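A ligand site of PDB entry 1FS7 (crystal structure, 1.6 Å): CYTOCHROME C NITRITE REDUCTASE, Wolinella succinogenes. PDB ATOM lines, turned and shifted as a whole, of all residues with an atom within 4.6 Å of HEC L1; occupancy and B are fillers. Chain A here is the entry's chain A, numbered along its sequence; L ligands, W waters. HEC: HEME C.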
ATOM      1  N   TYR A  74      18.111  -0.257 -28.590  1.00  0.00           N
ATOM      2  CA  TYR A  74      18.115   0.677 -27.467  1.00  0.00           C
ATOM      3  C   TYR A  74      16.720   1.277 -27.359  1.00  0.00           C
ATOM      4  O   TYR A  74      16.264   1.974 -28.261  1.00  0.00           O
ATOM      5  CB  TYR A  74      19.154   1.796 -27.679  1.00  0.00           C
ATOM      6  CG  TYR A  74      19.095   2.867 -26.603  1.00  0.00           C
ATOM      7  CD1 TYR A  74      19.277   2.542 -25.264  1.00  0.00           C
ATOM      8  CD2 TYR A  74      18.820   4.197 -26.935  1.00  0.00           C
ATOM      9  CE1 TYR A  74      19.170   3.513 -24.263  1.00  0.00           C
ATOM     10  CE2 TYR A  74      18.710   5.175 -25.950  1.00  0.00           C
ATOM     11  CZ  TYR A  74      18.892   4.827 -24.620  1.00  0.00           C
ATOM     12  OH  TYR A  74      18.767   5.792 -23.644  1.00  0.00           O
ATOM     13  N   ASN A  75      16.036   0.991 -26.256  1.00  0.00           N
ATOM     14  CA  ASN A  75      14.681   1.491 -26.047  1.00  0.00           C
ATOM     15  C   ASN A  75      14.617   2.340 -24.781  1.00  0.00           C
ATOM     16  O   ASN A  75      15.523   2.288 -23.943  1.00  0.00           O
ATOM     17  CB  ASN A  75      13.705   0.327 -25.908  1.00  0.00           C
ATOM     18  CG  ASN A  75      13.876  -0.723 -26.992  1.00  0.00           C
ATOM     19  OD1 ASN A  75      13.960  -1.919 -26.700  1.00  0.00           O
ATOM     20  ND2 ASN A  75      13.924  -0.282 -28.236  1.00  0.00           N
ATOM     21  N   ALA A  76      13.549   3.116 -24.648  1.00  0.00           N
ATOM     22  CA  ALA A  76      13.345   3.961 -23.483  1.00  0.00           C
ATOM     23  C   ALA A  76      12.994   3.063 -22.306  1.00  0.00           C
ATOM     24  O   ALA A  76      12.552   1.916 -22.488  1.00  0.00           O
ATOM     25  CB  ALA A  76      12.225   4.958 -23.742  1.00  0.00           C
ATOM     26  N   PRO A  77      13.155   3.564 -21.081  1.00  0.00           N
ATOM     27  CA  PRO A  77      12.834   2.764 -19.891  1.00  0.00           C
ATOM     28  C   PRO A  77      11.335   2.538 -19.759  1.00  0.00           C
ATOM     29  O   PRO A  77      10.539   3.370 -20.189  1.00  0.00           O
ATOM     30  CB  PRO A  77      13.341   3.631 -18.732  1.00  0.00           C
ATOM     31  CG  PRO A  77      14.335   4.577 -19.370  1.00  0.00           C
ATOM     32  CD  PRO A  77      13.697   4.882 -20.693  1.00  0.00           C
ATOM     33  N   ASP A  86      13.479  -7.420 -20.220  1.00  0.00           N
ATOM     34  CA  ASP A  86      14.047  -6.550 -21.236  1.00  0.00           C
ATOM     35  C   ASP A  86      15.546  -6.803 -21.363  1.00  0.00           C
ATOM     36  O   ASP A  86      16.118  -6.680 -22.446  1.00  0.00           O
ATOM     37  CB  ASP A  86      13.756  -5.077 -20.923  1.00  0.00           C
ATOM     38  CG  ASP A  86      12.296  -4.728 -21.149  1.00  0.00           C
ATOM     39  OD1 ASP A  86      11.629  -5.515 -21.861  1.00  0.00           O
ATOM     40  OD2 ASP A  86      11.808  -3.697 -20.654  1.00  0.00           O
ATOM     41  N   ASN A  87      16.175  -7.177 -20.252  1.00  0.00           N
ATOM     42  CA  ASN A  87      17.599  -7.493 -20.216  1.00  0.00           C
ATOM     43  C   ASN A  87      17.791  -8.695 -21.135  1.00  0.00           C
ATOM     44  O   ASN A  87      18.739  -8.753 -21.928  1.00  0.00           O
ATOM     45  CB  ASN A  87      18.001  -7.836 -18.777  1.00  0.00           C
ATOM     46  CG  ASN A  87      19.492  -8.014 -18.582  1.00  0.00           C
ATOM     47  OD1 ASN A  87      19.930  -9.025 -18.060  1.00  0.00           O
ATOM     48  ND2 ASN A  87      20.276  -7.012 -18.994  1.00  0.00           N
ATOM     49  N   THR A  90      16.616  -7.598 -25.151  1.00  0.00           N
ATOM     50  CA  THR A  90      17.435  -6.691 -25.951  1.00  0.00           C
ATOM     51  C   THR A  90      18.434  -7.423 -26.832  1.00  0.00           C
ATOM     52  O   THR A  90      19.076  -8.385 -26.402  1.00  0.00           O
ATOM     53  CB  THR A  90      18.203  -5.669 -25.074  1.00  0.00           C
ATOM     54  OG1 THR A  90      18.959  -4.809 -25.928  1.00  0.00           O
ATOM     55  CG2 THR A  90      19.140  -6.389 -24.104  1.00  0.00           C
ATOM     56  N   ARG A  92      21.122  -6.462 -27.541  1.00  0.00           N
ATOM     57  CA  ARG A  92      22.470  -6.250 -27.013  1.00  0.00           C
ATOM     58  C   ARG A  92      23.040  -7.479 -26.302  1.00  0.00           C
ATOM     59  O   ARG A  92      24.256  -7.699 -26.340  1.00  0.00           O
ATOM     60  CB  ARG A  92      22.497  -5.029 -26.074  1.00  0.00           C
ATOM     61  CG  ARG A  92      21.991  -3.741 -26.719  1.00  0.00           C
ATOM     62  CD  ARG A  92      22.579  -2.491 -26.055  1.00  0.00           C
ATOM     63  NE  ARG A  92      22.233  -2.336 -24.647  1.00  0.00           N
ATOM     64  CZ  ARG A  92      21.085  -1.831 -24.201  1.00  0.00           C
ATOM     65  NH1 ARG A  92      20.153  -1.427 -25.052  1.00  0.00           N
ATOM     66  NH2 ARG A  92      20.869  -1.709 -22.894  1.00  0.00           N
ATOM     67  N   THR A  93      22.191  -8.286 -25.670  1.00  0.00           N
ATOM     68  CA  THR A  93      22.697  -9.473 -24.972  1.00  0.00           C
ATOM     69  C   THR A  93      22.904 -10.658 -25.918  1.00  0.00           C
ATOM     70  O   THR A  93      23.397 -11.704 -25.515  1.00  0.00           O
ATOM     71  CB  THR A  93      21.778  -9.886 -23.793  1.00  0.00           C
ATOM     72  OG1 THR A  93      20.409  -9.898 -24.218  1.00  0.00           O
ATOM     73  CG2 THR A  93      21.950  -8.906 -22.640  1.00  0.00           C
ATOM     74  N   LEU A 104      27.904 -10.390 -23.989  1.00  0.00           N
ATOM     75  CA  LEU A 104      28.069  -9.651 -22.745  1.00  0.00           C
ATOM     76  C   LEU A 104      28.374 -10.479 -21.495  1.00  0.00           C
ATOM     77  O   LEU A 104      28.106 -11.677 -21.446  1.00  0.00           O
ATOM     78  CB  LEU A 104      26.841  -8.767 -22.528  1.00  0.00           C
ATOM     79  CG  LEU A 104      26.595  -7.830 -23.721  1.00  0.00           C
ATOM     80  CD1 LEU A 104      25.378  -6.961 -23.481  1.00  0.00           C
ATOM     81  CD2 LEU A 104      27.827  -6.967 -23.943  1.00  0.00           C
ATOM     82  N   ALA A 107      27.988  -9.123 -15.387  1.00  0.00           N
ATOM     83  CA  ALA A 107      27.649  -7.840 -14.781  1.00  0.00           C
ATOM     84  C   ALA A 107      26.375  -7.219 -15.330  1.00  0.00           C
ATOM     85  O   ALA A 107      25.799  -6.330 -14.713  1.00  0.00           O
ATOM     86  CB  ALA A 107      28.824  -6.861 -14.944  1.00  0.00           C
ATOM     87  N   CYS A 108      25.912  -7.683 -16.494  1.00  0.00           N
ATOM     88  CA  CYS A 108      24.689  -7.110 -17.063  1.00  0.00           C
ATOM     89  C   CYS A 108      23.422  -7.437 -16.269  1.00  0.00           C
ATOM     90  O   CYS A 108      22.392  -6.812 -16.492  1.00  0.00           O
ATOM     91  CB  CYS A 108      24.537  -7.528 -18.524  1.00  0.00           C
ATOM     92  SG  CYS A 108      25.583  -6.582 -19.659  1.00  0.00           S
ATOM     93  N   THR A 110      23.330  -7.312 -12.875  1.00  0.00           N
ATOM     94  CA  THR A 110      23.457  -6.483 -11.679  1.00  0.00           C
ATOM     95  C   THR A 110      22.324  -5.578 -11.233  1.00  0.00           C
ATOM     96  O   THR A 110      21.917  -5.627 -10.074  1.00  0.00           O
ATOM     97  CB  THR A 110      24.739  -5.639 -11.752  1.00  0.00           C
ATOM     98  OG1 THR A 110      25.843  -6.483 -12.125  1.00  0.00           O
ATOM     99  CG2 THR A 110      25.034  -5.006 -10.391  1.00  0.00           C
ATOM    100  N   CYS A 111      21.808  -4.754 -12.129  1.00  0.00           N
ATOM    101  CA  CYS A 111      20.743  -3.826 -11.771  1.00  0.00           C
ATOM    102  C   CYS A 111      19.383  -4.220 -12.342  1.00  0.00           C
ATOM    103  O   CYS A 111      18.567  -3.362 -12.666  1.00  0.00           O
ATOM    104  CB  CYS A 111      21.117  -2.428 -12.269  1.00  0.00           C
ATOM    105  SG  CYS A 111      22.809  -1.910 -11.804  1.00  0.00           S
ATOM    106  N   LYS A 112      19.130  -5.521 -12.421  1.00  0.00           N
ATOM    107  CA  LYS A 112      17.887  -6.013 -12.984  1.00  0.00           C
ATOM    108  C   LYS A 112      17.126  -6.990 -12.099  1.00  0.00           C
ATOM    109  O   LYS A 112      15.960  -7.300 -12.375  1.00  0.00           O
ATOM    110  CB  LYS A 112      18.190  -6.742 -14.311  1.00  0.00           C
ATOM    111  CG  LYS A 112      18.947  -5.925 -15.346  1.00  0.00           C
ATOM    112  CD  LYS A 112      18.078  -4.781 -15.870  1.00  0.00           C
ATOM    113  CE  LYS A 112      18.800  -3.986 -16.953  1.00  0.00           C
ATOM    114  NZ  LYS A 112      19.992  -3.253 -16.437  1.00  0.00           N
ATOM    115  N   TYR A 163      29.486  -1.575  -4.867  1.00  0.00           N
ATOM    116  CA  TYR A 163      30.061  -0.533  -5.720  1.00  0.00           C
ATOM    117  C   TYR A 163      29.499   0.855  -5.472  1.00  0.00           C
ATOM    118  O   TYR A 163      30.148   1.846  -5.795  1.00  0.00           O
ATOM    119  CB  TYR A 163      29.924  -0.911  -7.199  1.00  0.00           C
ATOM    120  CG  TYR A 163      28.509  -1.127  -7.702  1.00  0.00           C
ATOM    121  CD1 TYR A 163      27.655  -0.050  -7.923  1.00  0.00           C
ATOM    122  CD2 TYR A 163      28.042  -2.416  -7.976  1.00  0.00           C
ATOM    123  CE1 TYR A 163      26.363  -0.248  -8.411  1.00  0.00           C
ATOM    124  CE2 TYR A 163      26.759  -2.622  -8.457  1.00  0.00           C
ATOM    125  CZ  TYR A 163      25.927  -1.542  -8.675  1.00  0.00           C
ATOM    126  OH  TYR A 163      24.659  -1.747  -9.158  1.00  0.00           O
ATOM    127  N   GLN A 191      21.574   2.761  -6.674  1.00  0.00           N
ATOM    128  CA  GLN A 191      22.250   1.482  -6.786  1.00  0.00           C
ATOM    129  C   GLN A 191      22.293   1.116  -8.259  1.00  0.00           C
ATOM    130  O   GLN A 191      23.214   0.447  -8.732  1.00  0.00           O
ATOM    131  CB  GLN A 191      21.468   0.367  -6.090  1.00  0.00           C
ATOM    132  CG  GLN A 191      21.262   0.530  -4.617  1.00  0.00           C
ATOM    133  CD  GLN A 191      20.496  -0.649  -4.064  1.00  0.00           C
ATOM    134  OE1 GLN A 191      21.077  -1.715  -3.831  1.00  0.00           O
ATOM    135  NE2 GLN A 191      19.196  -0.473  -3.873  1.00  0.00           N
ATOM    136  N   CYS A 192      21.282   1.571  -8.999  1.00  0.00           N
ATOM    137  CA  CYS A 192      21.187   1.249 -10.415  1.00  0.00           C
ATOM    138  C   CYS A 192      21.127   2.424 -11.370  1.00  0.00           C
ATOM    139  O   CYS A 192      21.669   2.366 -12.471  1.00  0.00           O
ATOM    140  CB  CYS A 192      19.948   0.388 -10.644  1.00  0.00           C
ATOM    141  SG  CYS A 192      19.798  -1.018  -9.524  1.00  0.00           S
ATOM    142  N   HIS A 193      20.450   3.490 -10.954  1.00  0.00           N
ATOM    143  CA  HIS A 193      20.272   4.670 -11.797  1.00  0.00           C
ATOM    144  C   HIS A 193      21.462   5.616 -11.810  1.00  0.00           C
ATOM    145  O   HIS A 193      21.329   6.790 -11.441  1.00  0.00           O
ATOM    146  CB  HIS A 193      19.002   5.394 -11.360  1.00  0.00           C
ATOM    147  CG  HIS A 193      17.749   4.710 -11.789  1.00  0.00           C
ATOM    148  ND1 HIS A 193      17.136   4.923 -13.010  1.00  0.00           N
ATOM    149  CD2 HIS A 193      16.988   3.790 -11.157  1.00  0.00           C
ATOM    150  CE1 HIS A 193      16.050   4.129 -13.073  1.00  0.00           C
ATOM    151  NE2 HIS A 193      15.916   3.419 -11.966  1.00  0.00           N
ATOM    152  N   VAL A 194      22.609   5.096 -12.230  1.00  0.00           N
ATOM    153  CA  VAL A 194      23.847   5.863 -12.303  1.00  0.00           C
ATOM    154  C   VAL A 194      24.693   5.437 -13.497  1.00  0.00           C
ATOM    155  O   VAL A 194      24.414   4.414 -14.129  1.00  0.00           O
ATOM    156  CB  VAL A 194      24.707   5.648 -11.026  1.00  0.00           C
ATOM    157  CG1 VAL A 194      24.038   6.292  -9.822  1.00  0.00           C
ATOM    158  CG2 VAL A 194      24.901   4.159 -10.789  1.00  0.00           C
ATOM    159  N   TYR A 196      28.160   4.047 -15.190  1.00  0.00           N
ATOM    160  CA  TYR A 196      29.126   3.056 -14.733  1.00  0.00           C
ATOM    161  C   TYR A 196      29.976   2.565 -15.892  1.00  0.00           C
ATOM    162  O   TYR A 196      29.745   2.917 -17.047  1.00  0.00           O
ATOM    163  CB  TYR A 196      28.395   1.843 -14.164  1.00  0.00           C
ATOM    164  CG  TYR A 196      27.752   1.001 -15.263  1.00  0.00           C
ATOM    165  CD1 TYR A 196      26.542   1.387 -15.856  1.00  0.00           C
ATOM    166  CD2 TYR A 196      28.410  -0.115 -15.775  1.00  0.00           C
ATOM    167  CE1 TYR A 196      26.019   0.685 -16.942  1.00  0.00           C
ATOM    168  CE2 TYR A 196      27.887  -0.818 -16.862  1.00  0.00           C
ATOM    169  CZ  TYR A 196      26.706  -0.417 -17.447  1.00  0.00           C
ATOM    170  OH  TYR A 196      26.228  -1.097 -18.552  1.00  0.00           O
ATOM    171  N   PHE A 198      32.663  -1.156 -16.828  1.00  0.00           N
ATOM    172  CA  PHE A 198      33.165  -2.428 -16.324  1.00  0.00           C
ATOM    173  C   PHE A 198      34.677  -2.384 -16.219  1.00  0.00           C
ATOM    174  O   PHE A 198      35.369  -2.117 -17.203  1.00  0.00           O
ATOM    175  CB  PHE A 198      32.781  -3.588 -17.255  1.00  0.00           C
ATOM    176  CG  PHE A 198      31.293  -3.834 -17.361  1.00  0.00           C
ATOM    177  CD1 PHE A 198      30.449  -3.630 -16.271  1.00  0.00           C
ATOM    178  CD2 PHE A 198      30.752  -4.341 -18.541  1.00  0.00           C
ATOM    179  CE1 PHE A 198      29.092  -3.928 -16.351  1.00  0.00           C
ATOM    180  CE2 PHE A 198      29.393  -4.641 -18.635  1.00  0.00           C
ATOM    181  CZ  PHE A 198      28.565  -4.433 -17.533  1.00  0.00           C
ATOM    182  N   VAL A 216      31.431  -3.802 -11.982  1.00  0.00           N
ATOM    183  CA  VAL A 216      30.704  -2.544 -12.127  1.00  0.00           C
ATOM    184  C   VAL A 216      31.418  -1.511 -11.266  1.00  0.00           C
ATOM    185  O   VAL A 216      31.638  -1.734 -10.069  1.00  0.00           O
ATOM    186  CB  VAL A 216      29.244  -2.673 -11.641  1.00  0.00           C
ATOM    187  CG1 VAL A 216      28.581  -1.305 -11.614  1.00  0.00           C
ATOM    188  CG2 VAL A 216      28.475  -3.611 -12.563  1.00  0.00           C
ATOM    189  N   HIS A 255      22.478   6.002 -18.384  1.00  0.00           N
ATOM    190  CA  HIS A 255      21.572   6.513 -17.365  1.00  0.00           C
ATOM    191  C   HIS A 255      22.193   7.106 -16.098  1.00  0.00           C
ATOM    192  O   HIS A 255      22.110   6.510 -15.014  1.00  0.00           O
ATOM    193  CB  HIS A 255      20.599   5.392 -16.981  1.00  0.00           C
ATOM    194  CG  HIS A 255      21.240   4.045 -16.877  1.00  0.00           C
ATOM    195  ND1 HIS A 255      22.231   3.762 -15.957  1.00  0.00           N
ATOM    196  CD2 HIS A 255      21.088   2.915 -17.618  1.00  0.00           C
ATOM    197  CE1 HIS A 255      22.655   2.524 -16.132  1.00  0.00           C
ATOM    198  NE2 HIS A 255      21.981   1.992 -17.133  1.00  0.00           N
ATOM    199  N   ASP A 257      21.240   9.040 -14.051  1.00  0.00           N
ATOM    200  CA  ASP A 257      20.079   9.684 -13.441  1.00  0.00           C
ATOM    201  C   ASP A 257      20.374  10.400 -12.125  1.00  0.00           C
ATOM    202  O   ASP A 257      20.020  11.564 -11.953  1.00  0.00           O
ATOM    203  CB  ASP A 257      18.945   8.678 -13.221  1.00  0.00           C
ATOM    204  CG  ASP A 257      18.568   7.919 -14.494  1.00  0.00           C
ATOM    205  OD1 ASP A 257      18.323   8.566 -15.536  1.00  0.00           O
ATOM    206  OD2 ASP A 257      18.501   6.675 -14.431  1.00  0.00           O
ATOM    207  N   ALA A 376      21.338  10.399 -21.852  1.00  0.00           N
ATOM    208  CA  ALA A 376      21.225   9.017 -21.376  1.00  0.00           C
ATOM    209  C   ALA A 376      20.283   8.879 -20.189  1.00  0.00           C
ATOM    210  O   ALA A 376      19.684   7.822 -19.984  1.00  0.00           O
ATOM    211  CB  ALA A 376      22.601   8.464 -21.032  1.00  0.00           C
ATOM    212  N   HIS A 378      16.979   9.724 -19.086  1.00  0.00           N
ATOM    213  CA  HIS A 378      15.736  10.195 -19.698  1.00  0.00           C
ATOM    214  C   HIS A 378      14.927  11.246 -18.930  1.00  0.00           C
ATOM    215  O   HIS A 378      14.062  11.911 -19.507  1.00  0.00           O
ATOM    216  CB  HIS A 378      14.854   8.999 -20.034  1.00  0.00           C
ATOM    217  CG  HIS A 378      15.410   8.137 -21.127  1.00  0.00           C
ATOM    218  ND1 HIS A 378      15.232   8.433 -22.461  1.00  0.00           N
ATOM    219  CD2 HIS A 378      16.179   7.031 -21.076  1.00  0.00           C
ATOM    220  CE1 HIS A 378      15.885   7.535 -23.183  1.00  0.00           C
ATOM    221  NE2 HIS A 378      16.469   6.674 -22.371  1.00  0.00           N
HETATM  222 FE   HEC L   1      20.732  -1.786 -17.778  1.00  0.00          FE
HETATM  223  CHA HEC L   1      17.780  -0.266 -18.537  1.00  0.00           C
HETATM  224  CHB HEC L   1      20.375  -3.871 -20.443  1.00  0.00           C
HETATM  225  CHC HEC L   1      23.867  -2.990 -17.261  1.00  0.00           C
HETATM  226  CHD HEC L   1      20.892  -0.043 -14.891  1.00  0.00           C
HETATM  227  NA  HEC L   1      19.340  -2.041 -19.165  1.00  0.00           N
HETATM  228  C1A HEC L   1      18.181  -1.331 -19.341  1.00  0.00           C
HETATM  229  C2A HEC L   1      17.400  -1.855 -20.457  1.00  0.00           C
HETATM  230  C3A HEC L   1      18.115  -2.893 -20.972  1.00  0.00           C
HETATM  231  C4A HEC L   1      19.314  -3.000 -20.177  1.00  0.00           C
HETATM  232  CMA HEC L   1      17.757  -3.752 -22.185  1.00  0.00           C
HETATM  233  CAA HEC L   1      16.083  -1.275 -20.984  1.00  0.00           C
HETATM  234  CBA HEC L   1      16.352  -0.045 -21.841  1.00  0.00           C
HETATM  235  CGA HEC L   1      17.161  -0.360 -23.072  1.00  0.00           C
HETATM  236  O1A HEC L   1      16.592  -0.969 -24.001  1.00  0.00           O
HETATM  237  O2A HEC L   1      18.365  -0.029 -23.106  1.00  0.00           O
HETATM  238  NB  HEC L   1      21.871  -3.148 -18.675  1.00  0.00           N
HETATM  239  C1B HEC L   1      21.570  -3.927 -19.766  1.00  0.00           C
HETATM  240  C2B HEC L   1      22.721  -4.697 -20.212  1.00  0.00           C
HETATM  241  C3B HEC L   1      23.762  -4.395 -19.369  1.00  0.00           C
HETATM  242  C4B HEC L   1      23.185  -3.481 -18.371  1.00  0.00           C
HETATM  243  CMB HEC L   1      22.773  -5.641 -21.428  1.00  0.00           C
HETATM  244  CAB HEC L   1      25.104  -4.808 -19.484  1.00  0.00           C
HETATM  245  CBB HEC L   1      25.972  -4.165 -20.423  1.00  0.00           C
HETATM  246  NC  HEC L   1      22.125  -1.530 -16.391  1.00  0.00           N
HETATM  247  C1C HEC L   1      23.370  -2.105 -16.313  1.00  0.00           C
HETATM  248  C2C HEC L   1      24.019  -1.804 -15.038  1.00  0.00           C
HETATM  249  C3C HEC L   1      23.162  -1.017 -14.343  1.00  0.00           C
HETATM  250  C4C HEC L   1      22.007  -0.816 -15.214  1.00  0.00           C
HETATM  251  CMC HEC L   1      25.390  -2.317 -14.577  1.00  0.00           C
HETATM  252  CAC HEC L   1      23.277  -0.572 -12.997  1.00  0.00           C
HETATM  253  CBC HEC L   1      24.461   0.054 -12.502  1.00  0.00           C
HETATM  254  ND  HEC L   1      19.594  -0.420 -16.918  1.00  0.00           N
HETATM  255  C1D HEC L   1      19.776   0.186 -15.687  1.00  0.00           C
HETATM  256  C2D HEC L   1      18.794   1.245 -15.455  1.00  0.00           C
HETATM  257  C3D HEC L   1      18.009   1.274 -16.562  1.00  0.00           C
HETATM  258  C4D HEC L   1      18.472   0.195 -17.431  1.00  0.00           C
HETATM  259  CMD HEC L   1      18.661   2.140 -14.231  1.00  0.00           C
HETATM  260  CAD HEC L   1      16.818   2.227 -16.795  1.00  0.00           C
HETATM  261  CBD HEC L   1      17.130   3.658 -17.180  1.00  0.00           C
HETATM  262  CGD HEC L   1      17.556   3.811 -18.632  1.00  0.00           C
HETATM  263  O1D HEC L   1      17.619   2.800 -19.363  1.00  0.00           O
HETATM  264  O2D HEC L   1      17.846   4.948 -19.044  1.00  0.00           O
HETATM  265 FE   HEC L   2      14.392   2.126 -11.608  1.00  0.00          FE
HETATM  266  CHA HEC L   2      13.180   1.972 -14.806  1.00  0.00           C
HETATM  267  CHB HEC L   2      12.862   5.057 -11.173  1.00  0.00           C
HETATM  268  CHC HEC L   2      15.245   2.055  -8.339  1.00  0.00           C
HETATM  269  CHD HEC L   2      16.499  -0.416 -12.252  1.00  0.00           C
HETATM  270  NA  HEC L   2      13.183   3.210 -12.708  1.00  0.00           N
HETATM  271  C1A HEC L   2      12.702   2.980 -13.980  1.00  0.00           C
HETATM  272  C2A HEC L   2      11.815   4.048 -14.399  1.00  0.00           C
HETATM  273  C3A HEC L   2      11.780   4.958 -13.390  1.00  0.00           C
HETATM  274  C4A HEC L   2      12.631   4.432 -12.364  1.00  0.00           C
HETATM  275  CMA HEC L   2      10.962   6.239 -13.343  1.00  0.00           C
HETATM  276  CAA HEC L   2      10.981   4.145 -15.672  1.00  0.00           C
HETATM  277  CBA HEC L   2       9.600   3.536 -15.469  1.00  0.00           C
HETATM  278  CGA HEC L   2       8.690   3.729 -16.669  1.00  0.00           C
HETATM  279  O1A HEC L   2       9.199   4.100 -17.746  1.00  0.00           O
HETATM  280  O2A HEC L   2       7.474   3.484 -16.540  1.00  0.00           O
HETATM  281  NB  HEC L   2      14.081   3.312 -10.055  1.00  0.00           N
HETATM  282  C1B HEC L   2      13.495   4.538 -10.071  1.00  0.00           C
HETATM  283  C2B HEC L   2      13.511   5.151  -8.750  1.00  0.00           C
HETATM  284  C3B HEC L   2      14.117   4.267  -7.907  1.00  0.00           C
HETATM  285  C4B HEC L   2      14.469   3.130  -8.740  1.00  0.00           C
HETATM  286  CMB HEC L   2      12.898   6.510  -8.400  1.00  0.00           C
HETATM  287  CAB HEC L   2      14.299   4.381  -6.508  1.00  0.00           C
HETATM  288  CBB HEC L   2      13.192   4.560  -5.619  1.00  0.00           C
HETATM  289  NC  HEC L   2      15.590   1.037 -10.527  1.00  0.00           N
HETATM  290  C1C HEC L   2      15.772   1.084  -9.158  1.00  0.00           C
HETATM  291  C2C HEC L   2      16.706   0.086  -8.723  1.00  0.00           C
HETATM  292  C3C HEC L   2      17.135  -0.579  -9.827  1.00  0.00           C
HETATM  293  C4C HEC L   2      16.428   0.021 -10.941  1.00  0.00           C
HETATM  294  CMC HEC L   2      17.146  -0.180  -7.276  1.00  0.00           C
HETATM  295  CAC HEC L   2      18.106  -1.604  -9.860  1.00  0.00           C
HETATM  296  CBC HEC L   2      18.025  -2.781  -9.057  1.00  0.00           C
HETATM  297  ND  HEC L   2      14.785   1.052 -13.209  1.00  0.00           N
HETATM  298  C1D HEC L   2      15.716   0.033 -13.295  1.00  0.00           C
HETATM  299  C2D HEC L   2      15.658  -0.609 -14.583  1.00  0.00           C
HETATM  300  C3D HEC L   2      14.714   0.022 -15.301  1.00  0.00           C
HETATM  301  C4D HEC L   2      14.176   1.077 -14.460  1.00  0.00           C
HETATM  302  CMD HEC L   2      16.579  -1.732 -15.077  1.00  0.00           C
HETATM  303  CAD HEC L   2      14.349  -0.305 -16.740  1.00  0.00           C
HETATM  304  CBD HEC L   2      13.080  -1.152 -16.807  1.00  0.00           C
HETATM  305  CGD HEC L   2      12.773  -1.661 -18.212  1.00  0.00           C
HETATM  306  O1D HEC L   2      12.817  -0.841 -19.159  1.00  0.00           O
HETATM  307  O2D HEC L   2      12.491  -2.867 -18.371  1.00  0.00           O
HETATM  308  O   HOH W   1      15.556  -3.429 -18.224  1.00  0.00           O
HETATM  309  O   HOH W   2      17.288  -2.537 -26.181  1.00  0.00           O
HETATM  310  O   HOH W   3      17.025   7.250 -17.665  1.00  0.00           O
HETATM  311  O   HOH W   4      19.682   1.292 -20.901  1.00  0.00           O
HETATM  312  O   HOH W   5      14.290  -2.539 -23.825  1.00  0.00           O
HETATM  313  O   HOH W   6      21.581  -0.291 -18.857  1.00  0.00           O
HETATM  314  O   HOH W   7      23.782  -2.214 -22.092  1.00  0.00           O
HETATM  315  O   HOH W   8      19.364   5.489 -21.062  1.00  0.00           O
HETATM  316  O   HOH W   9      22.151  -4.678 -15.011  1.00  0.00           O
HETATM  317  O   HOH W  10      16.769   3.850 -21.949  1.00  0.00           O
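The side-chain amide nitrogen (ND2) of Asn 87 sits at hydrogen-bond distance from the backbone carbonyl oxygen (O) of Cys 108 (3.3 Å).
O of Val 194 sits at hydrogen-bond distance from ND1 of His 255 (2.9 Å).
O of Thr 90 lies within hydrogen-bond range of OG1 of Thr 93.
The side-chain hydroxyl (OG1) of Thr 93 lies within hydrogen-bond range of the backbone carbonyl oxygen (O) of Asn 87 (3.1 Å).
A ring nitrogen (NE2) of His 378 sits at hydrogen-bond distance from the side-chain hydroxyl (OH) of Tyr 74 (2.8 Å).
A ring nitrogen (ND1) of His 193 lies within hydrogen-bond range of the side-chain carboxylate (OD2) of Asp 257 (2.6 Å).
The side-chain hydroxyl of Tyr 163 is in hydrogen-bond range of the backbone carbonyl oxygen of Gln 191 (2.7 Å).
The side-chain hydroxyl (OH) of Tyr 163 lies within hydrogen-bond range of the side-chain sulfur (SG) of Cys 111 (3.2 Å).
Water W8 lies within hydrogen-bond range of O2D of HEC L1, O of Ala 376, OH of Tyr 74 and NE2 of His 378.
Water W2 lies within hydrogen-bond range of O1A of HEC L1 (2.8 Å), OG1 of Thr 90 (2.8 Å), NH1 of Arg 92 (3.3 Å), N of Tyr 74 (3.4 Å) and OD1 of Asn 75 (3.4 Å).
Water W5 bridges O1A of HEC L1 and OD1 of Asn 75.
Water W3 lies within hydrogen-bond range of O2D of HEC L1 (2.8 Å), OD1 of Asp 257 (2.8 Å) and N of His 378 (2.9 Å).
Water W10 lies within hydrogen-bond range of the backbone carbonyl oxygen of Asn 75, a ring nitrogen (NE2) of His 378, an oxygen (O1D) of HEC L1 and the side-chain hydroxyl of Tyr 74.
The side-chain carboxylate (OD2) of Asp 86 lies close to an oxygen (O2D) of HEC L2 (2.5 Å).
The side-chain sulfur (SG) of Cys 192 is covalently linked to a carbon (CAC) of HEC L2.
The side-chain amino group (NZ) of Lys 112 binds an iron atom (FE) of HEC L1 (2.1 Å).
CAB of HEC L1 is covalently linked to SG of Cys 108.
The guanidinium group (NH1) of Arg 92 lies within salt-bridge range of an oxygen (O2A) of HEC L1.
NE2 of His 193 is bound to FE of HEC L2 (2.0 Å).
O1A of HEC L1 lies within hydrogen-bond range of N of Asn 75 (3.0 Å).
CAC of HEC L1 is covalently linked to SG of Cys 111.
A nitrogen (ND) of HEC L1 lies close to a ring nitrogen (NE2) of His 255, 3.4 Å away.
CD1 of Tyr 74 touches O2A of HEC L1, at 3.5 Å.
CG of Pro 77 touches CGD of HEC L1, 3.4 Å away.
O of Asp 86 touches CMA of HEC L1 (3.4 Å).
ND2 of Asn 87 touches C1B of HEC L1, at 3.4 Å.
Thr 90 touches HEC L1 (CB to CMA, 3.5 Å).
Thr 93 touches HEC L1.
Leu 104 touches HEC L1 (CD1 to CMB, 3.6 Å).
Tyr 163 touches HEC L1 (OH to CBC, 3.8 Å).
O of Gln 191 touches CBC of HEC L1, at 3.99 Å.
O of Cys 192 touches CAC of HEC L1, 3.4 Å away.
ND1 of His 193 touches CMD of HEC L1 (3.4 Å).
Tyr 196 touches HEC L1.
Phe 198 touches HEC L1 (CE2 to CBB, 3.9 Å).
Val 216 touches HEC L1.
O of Ala 376 touches O2D of HEC L1 (3.5 Å).
His 378 touches HEC L1 (CD2 to O2D, 3.4 Å).
Of the 27 residues printed, 22 come within 4 Å of HEC L1.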
